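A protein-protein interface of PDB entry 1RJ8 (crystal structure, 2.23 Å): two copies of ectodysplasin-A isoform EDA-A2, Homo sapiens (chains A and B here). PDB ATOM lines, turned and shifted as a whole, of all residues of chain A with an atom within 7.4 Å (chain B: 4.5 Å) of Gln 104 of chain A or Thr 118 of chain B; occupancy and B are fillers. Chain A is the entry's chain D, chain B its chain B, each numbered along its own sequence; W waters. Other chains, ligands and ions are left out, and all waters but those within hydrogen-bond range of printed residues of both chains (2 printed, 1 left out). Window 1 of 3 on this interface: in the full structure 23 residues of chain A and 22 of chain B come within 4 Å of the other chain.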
ATOM      1  N   SER A  80     -11.160   3.582  -2.937  1.00  0.00           N
ATOM      2  CA  SER A  80     -11.554   2.732  -4.045  1.00  0.00           C
ATOM      3  C   SER A  80     -11.498   1.258  -3.657  1.00  0.00           C
ATOM      4  O   SER A  80     -10.879   0.873  -2.660  1.00  0.00           O
ATOM      5  CB  SER A  80     -10.643   2.985  -5.244  1.00  0.00           C
ATOM      6  OG  SER A  80      -9.332   2.525  -4.982  1.00  0.00           O
ATOM      7  N   TYR A  84     -11.245  -8.247  -7.946  1.00  0.00           N
ATOM      8  CA  TYR A  84     -10.508  -9.162  -8.810  1.00  0.00           C
ATOM      9  C   TYR A  84     -11.187 -10.523  -8.821  1.00  0.00           C
ATOM     10  O   TYR A  84     -11.247 -11.182  -7.790  1.00  0.00           O
ATOM     11  CB  TYR A  84      -9.067  -9.339  -8.318  1.00  0.00           C
ATOM     12  CG  TYR A  84      -8.243  -8.069  -8.199  1.00  0.00           C
ATOM     13  CD1 TYR A  84      -8.412  -7.005  -9.075  1.00  0.00           C
ATOM     14  CD2 TYR A  84      -7.253  -7.958  -7.224  1.00  0.00           C
ATOM     15  CE1 TYR A  84      -7.635  -5.858  -8.965  1.00  0.00           C
ATOM     16  CE2 TYR A  84      -6.478  -6.818  -7.109  1.00  0.00           C
ATOM     17  CZ  TYR A  84      -6.672  -5.769  -7.980  1.00  0.00           C
ATOM     18  OH  TYR A  84      -5.900  -4.628  -7.868  1.00  0.00           O
ATOM     19  N   PHE A  90      -0.467 -11.536 -11.070  1.00  0.00           N
ATOM     20  CA  PHE A  90      -0.288 -10.236 -10.455  1.00  0.00           C
ATOM     21  C   PHE A  90      -1.479  -9.358 -10.819  1.00  0.00           C
ATOM     22  O   PHE A  90      -1.690  -9.042 -11.990  1.00  0.00           O
ATOM     23  CB  PHE A  90       1.007  -9.615 -10.973  1.00  0.00           C
ATOM     24  CG  PHE A  90       1.354  -8.294 -10.351  1.00  0.00           C
ATOM     25  CD1 PHE A  90       2.047  -8.245  -9.156  1.00  0.00           C
ATOM     26  CD2 PHE A  90       1.018  -7.102 -10.982  1.00  0.00           C
ATOM     27  CE1 PHE A  90       2.390  -7.028  -8.584  1.00  0.00           C
ATOM     28  CE2 PHE A  90       1.366  -5.876 -10.425  1.00  0.00           C
ATOM     29  CZ  PHE A  90       2.050  -5.837  -9.225  1.00  0.00           C
ATOM     30  N   ALA A  91      -2.266  -8.990  -9.816  1.00  0.00           N
ATOM     31  CA  ALA A  91      -3.383  -8.079 -10.004  1.00  0.00           C
ATOM     32  C   ALA A  91      -3.117  -6.811  -9.214  1.00  0.00           C
ATOM     33  O   ALA A  91      -2.688  -6.872  -8.068  1.00  0.00           O
ATOM     34  CB  ALA A  91      -4.683  -8.727  -9.574  1.00  0.00           C
ATOM     35  N   SER A  92      -3.332  -5.663  -9.846  1.00  0.00           N
ATOM     36  CA  SER A  92      -3.019  -4.390  -9.226  1.00  0.00           C
ATOM     37  C   SER A  92      -3.701  -3.227  -9.954  1.00  0.00           C
ATOM     38  O   SER A  92      -3.989  -3.299 -11.154  1.00  0.00           O
ATOM     39  CB  SER A  92      -1.504  -4.172  -9.202  1.00  0.00           C
ATOM     40  OG  SER A  92      -1.153  -3.136  -8.305  1.00  0.00           O
ATOM     41  N   TYR A  93      -3.995  -2.174  -9.202  1.00  0.00           N
ATOM     42  CA  TYR A  93      -4.414  -0.908  -9.779  1.00  0.00           C
ATOM     43  C   TYR A  93      -3.841   0.265  -8.984  1.00  0.00           C
ATOM     44  O   TYR A  93      -3.431   0.124  -7.838  1.00  0.00           O
ATOM     45  CB  TYR A  93      -5.944  -0.818  -9.888  1.00  0.00           C
ATOM     46  CG  TYR A  93      -6.666  -0.647  -8.583  1.00  0.00           C
ATOM     47  CD1 TYR A  93      -6.784   0.601  -7.999  1.00  0.00           C
ATOM     48  CD2 TYR A  93      -7.225  -1.733  -7.925  1.00  0.00           C
ATOM     49  CE1 TYR A  93      -7.434   0.771  -6.801  1.00  0.00           C
ATOM     50  CE2 TYR A  93      -7.884  -1.571  -6.716  1.00  0.00           C
ATOM     51  CZ  TYR A  93      -7.984  -0.316  -6.160  1.00  0.00           C
ATOM     52  OH  TYR A  93      -8.639  -0.132  -4.958  1.00  0.00           O
ATOM     53  N   GLU A  94      -3.796   1.420  -9.629  1.00  0.00           N
ATOM     54  CA  GLU A  94      -3.398   2.665  -9.001  1.00  0.00           C
ATOM     55  C   GLU A  94      -4.581   3.632  -9.004  1.00  0.00           C
ATOM     56  O   GLU A  94      -5.398   3.626  -9.925  1.00  0.00           O
ATOM     57  CB  GLU A  94      -2.233   3.266  -9.775  1.00  0.00           C
ATOM     58  CG  GLU A  94      -0.948   2.460  -9.660  1.00  0.00           C
ATOM     59  CD  GLU A  94       0.162   2.975 -10.560  1.00  0.00           C
ATOM     60  OE1 GLU A  94      -0.122   3.741 -11.496  1.00  0.00           O
ATOM     61  OE2 GLU A  94       1.324   2.607 -10.325  1.00  0.00           O
ATOM     62  N   VAL A  95      -4.692   4.432  -7.949  1.00  0.00           N
ATOM     63  CA  VAL A  95      -5.545   5.603  -7.966  1.00  0.00           C
ATOM     64  C   VAL A  95      -4.635   6.773  -8.301  1.00  0.00           C
ATOM     65  O   VAL A  95      -3.739   7.106  -7.532  1.00  0.00           O
ATOM     66  CB  VAL A  95      -6.220   5.855  -6.603  1.00  0.00           C
ATOM     67  CG1 VAL A  95      -7.007   7.147  -6.633  1.00  0.00           C
ATOM     68  CG2 VAL A  95      -7.128   4.701  -6.226  1.00  0.00           C
ATOM     69  N   PRO A 101       0.547   8.462  -9.718  1.00  0.00           N
ATOM     70  CA  PRO A 101       0.174   7.476  -8.695  1.00  0.00           C
ATOM     71  C   PRO A 101       0.115   8.089  -7.284  1.00  0.00           C
ATOM     72  O   PRO A 101       1.055   8.756  -6.856  1.00  0.00           O
ATOM     73  CB  PRO A 101       1.288   6.424  -8.788  1.00  0.00           C
ATOM     74  CG  PRO A 101       1.896   6.596 -10.135  1.00  0.00           C
ATOM     75  CD  PRO A 101       1.749   8.049 -10.470  1.00  0.00           C
ATOM     76  N   PHE A 102      -1.003   7.874  -6.603  1.00  0.00           N
ATOM     77  CA  PHE A 102      -1.237   8.352  -5.235  1.00  0.00           C
ATOM     78  C   PHE A 102      -1.476   7.170  -4.296  1.00  0.00           C
ATOM     79  O   PHE A 102      -0.951   7.133  -3.177  1.00  0.00           O
ATOM     80  CB  PHE A 102      -2.451   9.297  -5.207  1.00  0.00           C
ATOM     81  CG  PHE A 102      -2.862   9.729  -3.823  1.00  0.00           C
ATOM     82  CD1 PHE A 102      -1.942  10.290  -2.957  1.00  0.00           C
ATOM     83  CD2 PHE A 102      -4.181   9.604  -3.399  1.00  0.00           C
ATOM     84  CE1 PHE A 102      -2.313  10.688  -1.679  1.00  0.00           C
ATOM     85  CE2 PHE A 102      -4.558  10.006  -2.118  1.00  0.00           C
ATOM     86  CZ  PHE A 102      -3.618  10.550  -1.263  1.00  0.00           C
ATOM     87  N   LEU A 103      -2.280   6.213  -4.761  1.00  0.00           N
ATOM     88  CA  LEU A 103      -2.596   4.996  -4.009  1.00  0.00           C
ATOM     89  C   LEU A 103      -2.454   3.758  -4.894  1.00  0.00           C
ATOM     90  O   LEU A 103      -2.416   3.856  -6.117  1.00  0.00           O
ATOM     91  CB  LEU A 103      -4.030   5.064  -3.471  1.00  0.00           C
ATOM     92  CG  LEU A 103      -4.402   6.291  -2.638  1.00  0.00           C
ATOM     93  CD1 LEU A 103      -5.912   6.367  -2.433  1.00  0.00           C
ATOM     94  CD2 LEU A 103      -3.694   6.261  -1.308  1.00  0.00           C
ATOM     95  N   GLN A 104      -2.379   2.593  -4.262  1.00  0.00           N
ATOM     96  CA  GLN A 104      -2.267   1.317  -4.969  1.00  0.00           C
ATOM     97  C   GLN A 104      -2.885   0.190  -4.143  1.00  0.00           C
ATOM     98  O   GLN A 104      -2.824   0.205  -2.912  1.00  0.00           O
ATOM     99  CB  GLN A 104      -0.795   1.001  -5.274  1.00  0.00           C
ATOM    100  CG  GLN A 104      -0.565  -0.302  -6.069  1.00  0.00           C
ATOM    101  CD  GLN A 104       0.864  -0.470  -6.569  1.00  0.00           C
ATOM    102  OE1 GLN A 104       1.532  -1.456  -6.247  1.00  0.00           O
ATOM    103  NE2 GLN A 104       1.325   0.474  -7.363  1.00  0.00           N
ATOM    104  N   CYS A 105      -3.483  -0.782  -4.826  1.00  0.00           N
ATOM    105  CA  CYS A 105      -3.949  -2.004  -4.185  1.00  0.00           C
ATOM    106  C   CYS A 105      -3.555  -3.199  -5.038  1.00  0.00           C
ATOM    107  O   CYS A 105      -3.832  -3.226  -6.233  1.00  0.00           O
ATOM    108  CB  CYS A 105      -5.457  -1.977  -3.981  1.00  0.00           C
ATOM    109  SG  CYS A 105      -6.028  -3.310  -2.901  1.00  0.00           S
ATOM    110  N   THR A 106      -2.913  -4.184  -4.420  1.00  0.00           N
ATOM    111  CA  THR A 106      -2.279  -5.278  -5.153  1.00  0.00           C
ATOM    112  C   THR A 106      -2.563  -6.638  -4.509  1.00  0.00           C
ATOM    113  O   THR A 106      -2.574  -6.761  -3.286  1.00  0.00           O
ATOM    114  CB  THR A 106      -0.757  -5.029  -5.212  1.00  0.00           C
ATOM    115  OG1 THR A 106      -0.495  -3.797  -5.897  1.00  0.00           O
ATOM    116  CG2 THR A 106      -0.041  -6.083  -6.035  1.00  0.00           C
ATOM    117  N   ARG A 107      -2.807  -7.643  -5.351  1.00  0.00           N
ATOM    118  CA  ARG A 107      -2.932  -9.043  -4.930  1.00  0.00           C
ATOM    119  C   ARG A 107      -2.060  -9.937  -5.802  1.00  0.00           C
ATOM    120  O   ARG A 107      -1.682  -9.572  -6.915  1.00  0.00           O
ATOM    121  CB  ARG A 107      -4.374  -9.545  -5.051  1.00  0.00           C
ATOM    122  CG  ARG A 107      -5.444  -8.739  -4.326  1.00  0.00           C
ATOM    123  CD  ARG A 107      -5.488  -8.923  -2.823  1.00  0.00           C
ATOM    124  NE  ARG A 107      -4.801  -7.823  -2.178  1.00  0.00           N
ATOM    125  CZ  ARG A 107      -5.335  -6.938  -1.347  1.00  0.00           C
ATOM    126  NH1 ARG A 107      -6.596  -6.995  -0.953  1.00  0.00           N
ATOM    127  NH2 ARG A 107      -4.559  -5.984  -0.884  1.00  0.00           N
ATOM    128  N   SER A 108      -1.781 -11.132  -5.302  1.00  0.00           N
ATOM    129  CA  SER A 108      -0.974 -12.101  -6.027  1.00  0.00           C
ATOM    130  C   SER A 108      -1.630 -13.478  -6.047  1.00  0.00           C
ATOM    131  O   SER A 108      -2.561 -13.765  -5.291  1.00  0.00           O
ATOM    132  CB  SER A 108       0.414 -12.213  -5.398  1.00  0.00           C
ATOM    133  OG  SER A 108       1.150 -11.026  -5.593  1.00  0.00           O
ATOM    134  N   CYS A 119     -10.203  -5.534  -3.289  1.00  0.00           N
ATOM    135  CA  CYS A 119      -8.920  -4.906  -3.120  1.00  0.00           C
ATOM    136  C   CYS A 119      -9.172  -3.429  -2.899  1.00  0.00           C
ATOM    137  O   CYS A 119      -9.379  -2.682  -3.838  1.00  0.00           O
ATOM    138  CB  CYS A 119      -8.051  -5.170  -4.354  1.00  0.00           C
ATOM    139  SG  CYS A 119      -6.293  -4.965  -4.052  1.00  0.00           S
ATOM    140  N   TYR A 120      -9.131  -3.025  -1.638  1.00  0.00           N
ATOM    141  CA  TYR A 120      -9.473  -1.673  -1.208  1.00  0.00           C
ATOM    142  C   TYR A 120      -8.222  -0.885  -0.831  1.00  0.00           C
ATOM    143  O   TYR A 120      -7.316  -1.419  -0.189  1.00  0.00           O
ATOM    144  CB  TYR A 120     -10.376  -1.763   0.027  1.00  0.00           C
ATOM    145  CG  TYR A 120     -10.778  -0.438   0.624  1.00  0.00           C
ATOM    146  CD1 TYR A 120      -9.921   0.263   1.475  1.00  0.00           C
ATOM    147  CD2 TYR A 120     -12.033   0.107   0.363  1.00  0.00           C
ATOM    148  CE1 TYR A 120     -10.305   1.483   2.035  1.00  0.00           C
ATOM    149  CE2 TYR A 120     -12.423   1.320   0.916  1.00  0.00           C
ATOM    150  CZ  TYR A 120     -11.558   2.002   1.746  1.00  0.00           C
ATOM    151  OH  TYR A 120     -11.966   3.193   2.295  1.00  0.00           O
ATOM    152  N   THR A 121      -8.187   0.381  -1.234  1.00  0.00           N
ATOM    153  CA  THR A 121      -7.214   1.337  -0.720  1.00  0.00           C
ATOM    154  C   THR A 121      -7.843   2.733  -0.571  1.00  0.00           C
ATOM    155  O   THR A 121      -8.878   3.026  -1.163  1.00  0.00           O
ATOM    156  CB  THR A 121      -5.951   1.381  -1.615  1.00  0.00           C
ATOM    157  OG1 THR A 121      -4.948   2.219  -1.017  1.00  0.00           O
ATOM    158  CG2 THR A 121      -6.243   2.018  -2.977  1.00  0.00           C
ATOM    159  N   ALA A 122      -7.218   3.571   0.247  1.00  0.00           N
ATOM    160  CA  ALA A 122      -7.716   4.922   0.510  1.00  0.00           C
ATOM    161  C   ALA A 122      -6.646   5.809   1.126  1.00  0.00           C
ATOM    162  O   ALA A 122      -5.745   5.326   1.809  1.00  0.00           O
ATOM    163  CB  ALA A 122      -8.919   4.864   1.443  1.00  0.00           C
ATOM    164  N   VAL A 138      -3.274  -1.855 -13.863  1.00  0.00           N
ATOM    165  CA  VAL A 138      -1.981  -2.121 -14.494  1.00  0.00           C
ATOM    166  C   VAL A 138      -2.178  -3.070 -15.675  1.00  0.00           C
ATOM    167  O   VAL A 138      -3.088  -3.897 -15.670  1.00  0.00           O
ATOM    168  CB  VAL A 138      -0.944  -2.716 -13.508  1.00  0.00           C
ATOM    169  CG1 VAL A 138      -0.686  -1.750 -12.357  1.00  0.00           C
ATOM    170  CG2 VAL A 138      -1.384  -4.090 -12.984  1.00  0.00           C
ATOM    171  N   GLN B  81      -1.326   1.650   5.117  1.00  0.00           N
ATOM    172  CA  GLN B  81      -1.141   0.591   4.141  1.00  0.00           C
ATOM    173  C   GLN B  81       0.328   0.204   4.061  1.00  0.00           C
ATOM    174  O   GLN B  81       1.201   1.066   4.014  1.00  0.00           O
ATOM    175  CB  GLN B  81      -1.618   1.032   2.770  1.00  0.00           C
ATOM    176  CG  GLN B  81      -1.603  -0.092   1.748  1.00  0.00           C
ATOM    177  CD  GLN B  81      -2.297   0.289   0.463  1.00  0.00           C
ATOM    178  OE1 GLN B  81      -3.522   0.381   0.425  1.00  0.00           O
ATOM    179  NE2 GLN B  81      -1.523   0.496  -0.596  1.00  0.00           N
ATOM    180  N   VAL B  82       0.589  -1.097   4.071  1.00  0.00           N
ATOM    181  CA  VAL B  82       1.931  -1.610   3.868  1.00  0.00           C
ATOM    182  C   VAL B  82       1.902  -2.491   2.632  1.00  0.00           C
ATOM    183  O   VAL B  82       1.051  -3.380   2.509  1.00  0.00           O
ATOM    184  CB  VAL B  82       2.426  -2.409   5.080  1.00  0.00           C
ATOM    185  CG1 VAL B  82       3.860  -2.894   4.872  1.00  0.00           C
ATOM    186  CG2 VAL B  82       2.356  -1.565   6.345  1.00  0.00           C
ATOM    187  N   TYR B  83       2.832  -2.240   1.717  1.00  0.00           N
ATOM    188  CA  TYR B  83       2.958  -3.046   0.512  1.00  0.00           C
ATOM    189  C   TYR B  83       3.946  -4.185   0.746  1.00  0.00           C
ATOM    190  O   TYR B  83       5.158  -4.002   0.680  1.00  0.00           O
ATOM    191  CB  TYR B  83       3.373  -2.187  -0.691  1.00  0.00           C
ATOM    192  CG  TYR B  83       3.397  -2.916  -2.025  1.00  0.00           C
ATOM    193  CD1 TYR B  83       2.594  -4.028  -2.252  1.00  0.00           C
ATOM    194  CD2 TYR B  83       4.211  -2.479  -3.069  1.00  0.00           C
ATOM    195  CE1 TYR B  83       2.602  -4.692  -3.469  1.00  0.00           C
ATOM    196  CE2 TYR B  83       4.233  -3.140  -4.299  1.00  0.00           C
ATOM    197  CZ  TYR B  83       3.418  -4.245  -4.490  1.00  0.00           C
ATOM    198  OH  TYR B  83       3.418  -4.903  -5.689  1.00  0.00           O
ATOM    199  N   ARG B 107      -2.081 -10.993   6.350  1.00  0.00           N
ATOM    200  CA  ARG B 107      -2.132 -11.742   5.097  1.00  0.00           C
ATOM    201  C   ARG B 107      -1.395 -13.056   5.314  1.00  0.00           C
ATOM    202  O   ARG B 107      -0.367 -13.099   5.991  1.00  0.00           O
ATOM    203  CB  ARG B 107      -1.414 -11.005   3.961  1.00  0.00           C
ATOM    204  CG  ARG B 107      -1.957  -9.652   3.549  1.00  0.00           C
ATOM    205  CD  ARG B 107      -3.194  -9.686   2.664  1.00  0.00           C
ATOM    206  NE  ARG B 107      -4.334  -9.326   3.480  1.00  0.00           N
ATOM    207  CZ  ARG B 107      -5.036  -8.202   3.402  1.00  0.00           C
ATOM    208  NH1 ARG B 107      -4.807  -7.266   2.485  1.00  0.00           N
ATOM    209  NH2 ARG B 107      -6.015  -8.038   4.261  1.00  0.00           N
ATOM    210  N   ASN B 117       1.431  -7.931  -2.244  1.00  0.00           N
ATOM    211  CA  ASN B 117       0.145  -7.760  -1.587  1.00  0.00           C
ATOM    212  C   ASN B 117       0.113  -6.553  -0.644  1.00  0.00           C
ATOM    213  O   ASN B 117       0.921  -6.464   0.276  1.00  0.00           O
ATOM    214  CB  ASN B 117      -0.207  -9.050  -0.844  1.00  0.00           C
ATOM    215  CG  ASN B 117      -1.544  -8.984  -0.180  1.00  0.00           C
ATOM    216  OD1 ASN B 117      -1.765  -8.131   0.667  1.00  0.00           O
ATOM    217  ND2 ASN B 117      -2.452  -9.882  -0.557  1.00  0.00           N
ATOM    218  N   THR B 118      -0.819  -5.629  -0.887  1.00  0.00           N
ATOM    219  CA  THR B 118      -1.003  -4.473  -0.018  1.00  0.00           C
ATOM    220  C   THR B 118      -2.007  -4.795   1.065  1.00  0.00           C
ATOM    221  O   THR B 118      -2.987  -5.491   0.838  1.00  0.00           O
ATOM    222  CB  THR B 118      -1.485  -3.234  -0.790  1.00  0.00           C
ATOM    223  OG1 THR B 118      -2.691  -3.537  -1.499  1.00  0.00           O
ATOM    224  CG2 THR B 118      -0.471  -2.812  -1.871  1.00  0.00           C
ATOM    225  N   CYS B 119      -1.770  -4.258   2.245  1.00  0.00           N
ATOM    226  CA  CYS B 119      -2.560  -4.592   3.406  1.00  0.00           C
ATOM    227  C   CYS B 119      -2.990  -3.294   4.064  1.00  0.00           C
ATOM    228  O   CYS B 119      -2.191  -2.639   4.716  1.00  0.00           O
ATOM    229  CB  CYS B 119      -1.724  -5.446   4.357  1.00  0.00           C
ATOM    230  SG  CYS B 119      -2.720  -6.435   5.482  1.00  0.00           S
ATOM    231  N   TYR B 120      -4.251  -2.920   3.873  1.00  0.00           N
ATOM    232  CA  TYR B 120      -4.773  -1.659   4.385  1.00  0.00           C
ATOM    233  C   TYR B 120      -5.651  -1.900   5.616  1.00  0.00           C
ATOM    234  O   TYR B 120      -6.419  -2.857   5.669  1.00  0.00           O
ATOM    235  CB  TYR B 120      -5.581  -0.954   3.290  1.00  0.00           C
ATOM    236  CG  TYR B 120      -6.245   0.340   3.703  1.00  0.00           C
ATOM    237  CD1 TYR B 120      -7.419   0.337   4.463  1.00  0.00           C
ATOM    238  CD2 TYR B 120      -5.723   1.573   3.315  1.00  0.00           C
ATOM    239  CE1 TYR B 120      -8.040   1.521   4.839  1.00  0.00           C
ATOM    240  CE2 TYR B 120      -6.345   2.768   3.691  1.00  0.00           C
ATOM    241  CZ  TYR B 120      -7.504   2.733   4.452  1.00  0.00           C
ATOM    242  OH  TYR B 120      -8.143   3.903   4.818  1.00  0.00           O
ATOM    243  N   HIS B 149       3.145   5.664  -3.062  1.00  0.00           N
ATOM    244  CA  HIS B 149       1.758   5.284  -3.361  1.00  0.00           C
ATOM    245  C   HIS B 149       1.371   3.872  -2.911  1.00  0.00           C
ATOM    246  O   HIS B 149       0.217   3.474  -3.086  1.00  0.00           O
ATOM    247  CB  HIS B 149       1.479   5.433  -4.856  1.00  0.00           C
ATOM    248  CG  HIS B 149       2.500   4.778  -5.730  1.00  0.00           C
ATOM    249  ND1 HIS B 149       2.352   3.499  -6.223  1.00  0.00           N
ATOM    250  CD2 HIS B 149       3.685   5.229  -6.199  1.00  0.00           C
ATOM    251  CE1 HIS B 149       3.406   3.191  -6.957  1.00  0.00           C
ATOM    252  NE2 HIS B 149       4.230   4.224  -6.958  1.00  0.00           N
ATOM    253  N   THR B 150       2.311   3.122  -2.332  1.00  0.00           N
ATOM    254  CA  THR B 150       2.046   1.732  -1.931  1.00  0.00           C
ATOM    255  C   THR B 150       2.062   1.518  -0.419  1.00  0.00           C
ATOM    256  O   THR B 150       1.300   0.702   0.104  1.00  0.00           O
ATOM    257  CB  THR B 150       3.052   0.760  -2.605  1.00  0.00           C
ATOM    258  OG1 THR B 150       4.378   0.995  -2.114  1.00  0.00           O
ATOM    259  CG2 THR B 150       3.145   1.006  -4.096  1.00  0.00           C
HETATM  260  O   HOH W   1      -6.141  -3.827   1.184  1.00  0.00           O
HETATM  261  O   HOH W   2     -10.945   3.721   4.913  1.00  0.00           O
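OG1 of Thr 118 of chain B sits at hydrogen-bond distance from NH2 of Arg 107 of chain A (3.1 Å).
The side-chain hydroxyl (OG1) of Thr 121 of chain A sits at hydrogen-bond distance from the side-chain amide oxygen (OE1) of Gln 81 of chain B (2.7 Å).
The backbone NH (N) of Gln 104 of chain A lies within hydrogen-bond range of the backbone carbonyl oxygen (O) of His 149 of chain B (3.0 Å).
The side-chain sulfur (SG) of Cys 105 of chain A lies close to the side-chain hydroxyl (OG1) of Thr 118 of chain B (3.6 Å).
The side-chain amide nitrogen (NE2) of Gln 81 of chain B is in hydrogen-bond range of the backbone carbonyl oxygen (O) of Gln 104 of chain A.
N of Thr 106 of chain A sits at hydrogen-bond distance from OG1 of Thr 118 of chain B, 3.0 Å away.
The guanidinium group (NH1) of Arg 107 of chain B is in hydrogen-bond range of the backbone carbonyl oxygen (O) of Thr 118 of chain B (3.0 Å).
The backbone carbonyl oxygen (O) of Ala 91 of chain A sits at hydrogen-bond distance from the backbone NH (N) of Arg 107 of chain A, 2.8 Å away.
OE1 of Gln 104 of chain A is in hydrogen-bond range of OG1 of Thr 106 of chain A, 3.1 Å away.
O of Gln 104 of chain A lies within hydrogen-bond range of OG1 of Thr 121 of chain A (3.5 Å).
The backbone NH (N) of Phe 102 of chain A lies within hydrogen-bond range of the backbone carbonyl oxygen (O) of Val 95 of chain A, 3.0 Å away.
The backbone NH (N) of Val 95 of chain A is in hydrogen-bond range of the backbone carbonyl oxygen (O) of Leu 103 of chain A (3.0 Å).
CB of Pro 101 of chain A touches CG of His 149 of chain B (3.7 Å).
Phe 102 of chain A touches His 149 of chain B (O to CA, 3.3 Å).
His 149 of chain B touches Leu 103 of chain A (O to C, 3.2 Å).
Gln 104 of chain A touches Tyr 83 of chain B (OE1 to CE2, 3.7 Å).
Gln 104 of chain A touches Thr 118 of chain B (O to CG2, 3.97 Å).
Thr 106 of chain A touches Tyr 83 of chain B (CG2 to OH, 3.7 Å).
Arg 107 of chain A touches Arg 107 of chain B (NH2 to NH1, 3.6 Å).
Arg 107 of chain A touches Asn 117 of chain B.
Tyr 120 of chain A touches Tyr 120 of chain B (CE1 to CE1, 3.6 Å).
Ala 122 of chain A touches Tyr 120 of chain B (O to CE2, 3.2 Å).
Of chain A, only Gln 104, Cys 105, Thr 106 and Arg 107 come within 4 Å of Thr 118 of chain B.
Of the printed residues of chain B, Ala 122 of chain A touches Tyr 120.
Printed residues of chain B within 4 Å of Phe 90 of chain A: Tyr 83 (3.7 Å).
Val 95 of chain A touches none of the printed residues of chain B.
The nearest printed residue of chain B that does not touch Gln 104 of chain A is Tyr 120 of chain B (6.9 Å).
The nearest residue of chain A that does not touch Thr 118 of chain B is Cys 119 of chain A (4.6 Å).
Printed residues of chain A that touch a printed residue of chain B: Phe 90, Pro 101, Phe 102, Leu 103, Gln 104, Cys 105, Thr 106, Arg 107, Tyr 120, Thr 121 and Ala 122.
Hydrophobic or aromatic side chains of chain B that line the printed part of chain A: Tyr 83, Tyr 120 and His 149.
Among the printed residues, 19 pairs touch across the chains.
Among the printed residues, no Asp or Glu carboxylate lies within 4 Å of a Lys or Arg side-chain nitrogen of the other chain.
Arg 107 of chain B touches its own counterpart, Arg 107 of chain A.
Tyr 120 of chain A touches its own counterpart, Tyr 120 of chain B.
Positions printed for both chains: 107, 119 and 120.
Of the 19 pairs that touch across the chains among the printed residues, 2 have their exchanged pair printed and touching as well.
Water W2 lies within hydrogen-bond range of the side-chain hydroxyl of Tyr 120 of chain B (2.8 Å) and the side-chain hydroxyl of Tyr 120 of chain A (2.9 Å).
Water W1 lies within hydrogen-bond range of the backbone carbonyl oxygen (O) of Tyr 120 of chain A, the guanidinium group (NH2) of Arg 107 of chain A and the backbone NH (N) of Tyr 120 of chain B.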
